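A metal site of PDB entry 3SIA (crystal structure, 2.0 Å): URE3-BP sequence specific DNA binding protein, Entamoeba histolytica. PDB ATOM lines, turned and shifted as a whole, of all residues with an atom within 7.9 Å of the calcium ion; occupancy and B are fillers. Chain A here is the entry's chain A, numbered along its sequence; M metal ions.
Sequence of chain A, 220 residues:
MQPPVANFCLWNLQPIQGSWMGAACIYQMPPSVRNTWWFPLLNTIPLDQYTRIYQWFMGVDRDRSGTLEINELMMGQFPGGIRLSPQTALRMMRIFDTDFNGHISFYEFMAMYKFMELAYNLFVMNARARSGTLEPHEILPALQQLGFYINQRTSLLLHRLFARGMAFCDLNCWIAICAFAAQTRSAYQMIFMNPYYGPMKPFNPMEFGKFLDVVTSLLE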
ATOM      1  N   PHE A  57      -5.643  13.769 -15.485  1.00  0.00           N
ATOM      2  CA  PHE A  57      -5.305  14.123 -16.870  1.00  0.00           C
ATOM      3  C   PHE A  57      -5.815  15.527 -17.192  1.00  0.00           C
ATOM      4  O   PHE A  57      -5.089  16.317 -17.728  1.00  0.00           O
ATOM      5  CB  PHE A  57      -5.969  13.114 -17.810  1.00  0.00           C
ATOM      6  CG  PHE A  57      -5.621  13.276 -19.267  1.00  0.00           C
ATOM      7  CD1 PHE A  57      -4.404  12.841 -19.775  1.00  0.00           C
ATOM      8  CD2 PHE A  57      -6.579  13.771 -20.161  1.00  0.00           C
ATOM      9  CE1 PHE A  57      -4.131  12.928 -21.168  1.00  0.00           C
ATOM     10  CE2 PHE A  57      -6.300  13.873 -21.520  1.00  0.00           C
ATOM     11  CZ  PHE A  57      -5.052  13.457 -22.009  1.00  0.00           C
ATOM     12  N   VAL A  60      -3.644  18.199 -15.685  1.00  0.00           N
ATOM     13  CA  VAL A  60      -2.369  18.432 -16.344  1.00  0.00           C
ATOM     14  C   VAL A  60      -2.536  19.051 -17.775  1.00  0.00           C
ATOM     15  O   VAL A  60      -1.733  19.847 -18.221  1.00  0.00           O
ATOM     16  CB  VAL A  60      -1.582  17.097 -16.420  1.00  0.00           C
ATOM     17  CG1 VAL A  60      -0.218  17.325 -17.034  1.00  0.00           C
ATOM     18  CG2 VAL A  60      -1.495  16.494 -15.018  1.00  0.00           C
ATOM     19  N   ASP A  61      -3.596  18.670 -18.472  1.00  0.00           N
ATOM     20  CA  ASP A  61      -3.913  19.196 -19.809  1.00  0.00           C
ATOM     21  C   ASP A  61      -4.414  20.681 -19.777  1.00  0.00           C
ATOM     22  O   ASP A  61      -5.633  20.979 -19.943  1.00  0.00           O
ATOM     23  CB  ASP A  61      -4.953  18.277 -20.455  1.00  0.00           C
ATOM     24  CG  ASP A  61      -5.328  18.693 -21.869  1.00  0.00           C
ATOM     25  OD1 ASP A  61      -4.616  19.495 -22.501  1.00  0.00           O
ATOM     26  OD2 ASP A  61      -6.375  18.234 -22.341  1.00  0.00           O
ATOM     27  N   ARG A  62      -3.450  21.581 -19.651  1.00  0.00           N
ATOM     28  CA  ARG A  62      -3.705  23.003 -19.534  1.00  0.00           C
ATOM     29  C   ARG A  62      -4.407  23.675 -20.746  1.00  0.00           C
ATOM     30  O   ARG A  62      -5.094  24.649 -20.541  1.00  0.00           O
ATOM     31  CB  ARG A  62      -2.360  23.735 -19.198  1.00  0.00           C
ATOM     32  N   ASP A  63      -4.244  23.200 -21.975  1.00  0.00           N
ATOM     33  CA  ASP A  63      -4.965  23.784 -23.134  1.00  0.00           C
ATOM     34  C   ASP A  63      -6.245  23.010 -23.592  1.00  0.00           C
ATOM     35  O   ASP A  63      -6.808  23.284 -24.644  1.00  0.00           O
ATOM     36  CB  ASP A  63      -3.990  24.012 -24.303  1.00  0.00           C
ATOM     37  CG  ASP A  63      -3.382  22.753 -24.837  1.00  0.00           C
ATOM     38  OD1 ASP A  63      -3.692  21.655 -24.319  1.00  0.00           O
ATOM     39  OD2 ASP A  63      -2.604  22.866 -25.805  1.00  0.00           O
ATOM     40  N   ARG A  64      -6.701  22.068 -22.749  1.00  0.00           N
ATOM     41  CA  ARG A  64      -7.861  21.194 -23.010  1.00  0.00           C
ATOM     42  C   ARG A  64      -7.828  20.501 -24.394  1.00  0.00           C
ATOM     43  O   ARG A  64      -8.857  20.304 -25.014  1.00  0.00           O
ATOM     44  CB  ARG A  64      -9.141  21.937 -22.785  1.00  0.00           C
ATOM     45  CG  ARG A  64      -9.214  22.647 -21.401  1.00  0.00           C
ATOM     46  CD  ARG A  64     -10.609  23.313 -21.157  1.00  0.00           C
ATOM     47  NE  ARG A  64     -11.676  22.380 -21.559  1.00  0.00           N
ATOM     48  CZ  ARG A  64     -12.644  22.636 -22.442  1.00  0.00           C
ATOM     49  NH1 ARG A  64     -12.769  23.817 -23.015  1.00  0.00           N
ATOM     50  NH2 ARG A  64     -13.522  21.674 -22.721  1.00  0.00           N
ATOM     51  N   SER A  65      -6.632  20.153 -24.867  1.00  0.00           N
ATOM     52  CA  SER A  65      -6.498  19.503 -26.169  1.00  0.00           C
ATOM     53  C   SER A  65      -6.883  18.019 -26.126  1.00  0.00           C
ATOM     54  O   SER A  65      -7.031  17.370 -27.166  1.00  0.00           O
ATOM     55  CB  SER A  65      -5.069  19.613 -26.699  1.00  0.00           C
ATOM     56  OG  SER A  65      -4.162  18.874 -25.896  1.00  0.00           O
ATOM     57  N   GLY A  66      -7.048  17.474 -24.937  1.00  0.00           N
ATOM     58  CA  GLY A  66      -7.352  16.042 -24.862  1.00  0.00           C
ATOM     59  C   GLY A  66      -6.057  15.248 -24.946  1.00  0.00           C
ATOM     60  O   GLY A  66      -6.092  14.027 -25.132  1.00  0.00           O
ATOM     61  N   THR A  67      -4.934  15.963 -24.842  1.00  0.00           N
ATOM     62  CA  THR A  67      -3.629  15.363 -24.898  1.00  0.00           C
ATOM     63  C   THR A  67      -2.638  16.107 -24.006  1.00  0.00           C
ATOM     64  O   THR A  67      -2.828  17.267 -23.662  1.00  0.00           O
ATOM     65  CB  THR A  67      -3.082  15.311 -26.340  1.00  0.00           C
ATOM     66  OG1 THR A  67      -2.875  16.620 -26.833  1.00  0.00           O
ATOM     67  CG2 THR A  67      -4.031  14.565 -27.280  1.00  0.00           C
ATOM     68  N   LEU A  68      -1.574  15.443 -23.661  1.00  0.00           N
ATOM     69  CA  LEU A  68      -0.505  16.085 -22.872  1.00  0.00           C
ATOM     70  C   LEU A  68       0.752  16.286 -23.728  1.00  0.00           C
ATOM     71  O   LEU A  68       1.232  15.386 -24.401  1.00  0.00           O
ATOM     72  CB  LEU A  68      -0.169  15.261 -21.630  1.00  0.00           C
ATOM     73  CG  LEU A  68      -1.337  14.950 -20.689  1.00  0.00           C
ATOM     74  CD1 LEU A  68      -0.848  14.177 -19.472  1.00  0.00           C
ATOM     75  CD2 LEU A  68      -2.152  16.178 -20.249  1.00  0.00           C
ATOM     76  N   GLU A  69       1.275  17.498 -23.664  1.00  0.00           N
ATOM     77  CA  GLU A  69       2.474  17.869 -24.340  1.00  0.00           C
ATOM     78  C   GLU A  69       3.595  18.013 -23.337  1.00  0.00           C
ATOM     79  O   GLU A  69       3.363  18.031 -22.132  1.00  0.00           O
ATOM     80  CB  GLU A  69       2.236  19.202 -25.081  1.00  0.00           C
ATOM     81  CG  GLU A  69       1.387  19.028 -26.315  1.00  0.00           C
ATOM     82  CD  GLU A  69      -0.050  18.625 -25.999  1.00  0.00           C
ATOM     83  OE1 GLU A  69      -0.735  19.406 -25.295  1.00  0.00           O
ATOM     84  OE2 GLU A  69      -0.519  17.563 -26.505  1.00  0.00           O
ATOM     85  N   ILE A  70       4.816  18.142 -23.810  1.00  0.00           N
ATOM     86  CA  ILE A  70       5.968  18.083 -22.887  1.00  0.00           C
ATOM     87  C   ILE A  70       5.932  19.240 -21.867  1.00  0.00           C
ATOM     88  O   ILE A  70       6.210  19.027 -20.654  1.00  0.00           O
ATOM     89  CB  ILE A  70       7.298  18.073 -23.644  1.00  0.00           C
ATOM     90  CG1 ILE A  70       8.439  17.870 -22.655  1.00  0.00           C
ATOM     91  CG2 ILE A  70       7.418  19.344 -24.603  1.00  0.00           C
ATOM     92  CD1 ILE A  70       9.708  17.482 -23.315  1.00  0.00           C
ATOM     93  N   GLU A  72       3.309  20.584 -20.616  1.00  0.00           N
ATOM     94  CA  GLU A  72       2.318  20.177 -19.576  1.00  0.00           C
ATOM     95  C   GLU A  72       2.870  19.170 -18.572  1.00  0.00           C
ATOM     96  O   GLU A  72       2.537  19.225 -17.364  1.00  0.00           O
ATOM     97  CB  GLU A  72       1.003  19.675 -20.206  1.00  0.00           C
ATOM     98  CG  GLU A  72       0.250  20.811 -20.906  1.00  0.00           C
ATOM     99  CD  GLU A  72      -0.807  20.348 -21.881  1.00  0.00           C
ATOM    100  OE1 GLU A  72      -0.787  19.162 -22.258  1.00  0.00           O
ATOM    101  OE2 GLU A  72      -1.670  21.183 -22.304  1.00  0.00           O
ATOM    102  N   HIS A 103       2.579  14.051 -28.527  1.00  0.00           N
ATOM    103  CA  HIS A 103       1.415  14.092 -27.645  1.00  0.00           C
ATOM    104  C   HIS A 103       1.336  12.782 -26.846  1.00  0.00           C
ATOM    105  O   HIS A 103       1.655  11.704 -27.378  1.00  0.00           O
ATOM    106  CB  HIS A 103       0.139  14.247 -28.462  1.00  0.00           C
ATOM    107  CG  HIS A 103       0.138  15.437 -29.356  1.00  0.00           C
ATOM    108  ND1 HIS A 103       0.133  16.726 -28.859  1.00  0.00           N
ATOM    109  CD2 HIS A 103       0.184  15.552 -30.699  1.00  0.00           C
ATOM    110  CE1 HIS A 103       0.196  17.577 -29.869  1.00  0.00           C
ATOM    111  NE2 HIS A 103       0.219  16.895 -30.992  1.00  0.00           N
ATOM    112  N   ILE A 104       0.911  12.874 -25.599  1.00  0.00           N
ATOM    113  CA  ILE A 104       0.494  11.702 -24.834  1.00  0.00           C
ATOM    114  C   ILE A 104      -1.056  11.702 -24.811  1.00  0.00           C
ATOM    115  O   ILE A 104      -1.677  12.625 -24.302  1.00  0.00           O
ATOM    116  CB  ILE A 104       1.125  11.763 -23.395  1.00  0.00           C
ATOM    117  CG1 ILE A 104       2.562  11.251 -23.476  1.00  0.00           C
ATOM    118  CG2 ILE A 104       0.333  10.902 -22.351  1.00  0.00           C
ATOM    119  CD1 ILE A 104       3.268  11.501 -22.236  1.00  0.00           C
HETATM  120 CA    CA M   1      -2.779  19.503 -23.882  1.00  0.00          CA
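OE2 of Glu 69 sits at hydrogen-bond distance from ND1 of His 103 (2.6 Å). The side-chain carboxylate (OE2) of Glu 72 lies close to the backbone NH (N) of Arg 62 (3.2 Å). The side-chain carboxylate (OD2) of Asp 61 is in hydrogen-bond range of the backbone NH (N) of Gly 66 (2.8 Å). The backbone NH (N) of Arg 64 sits close to the side-chain carboxylate (OD1) of Asp 61 (3.3 Å).
Of the 15 residues printed, 6 come within 4 Å of the calcium ion.
The calcium ion is bound by O of Thr 67 (2.2 Å), OD1 of Asp 61 (2.3 Å), OD1 of Asp 63 (2.4 Å), OE1 of Glu 69 (2.5 Å), OG of Ser 65 (2.5 Å), OE2 of Glu 72 (2.6 Å) and OE1 of Glu 72 (2.6 Å).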
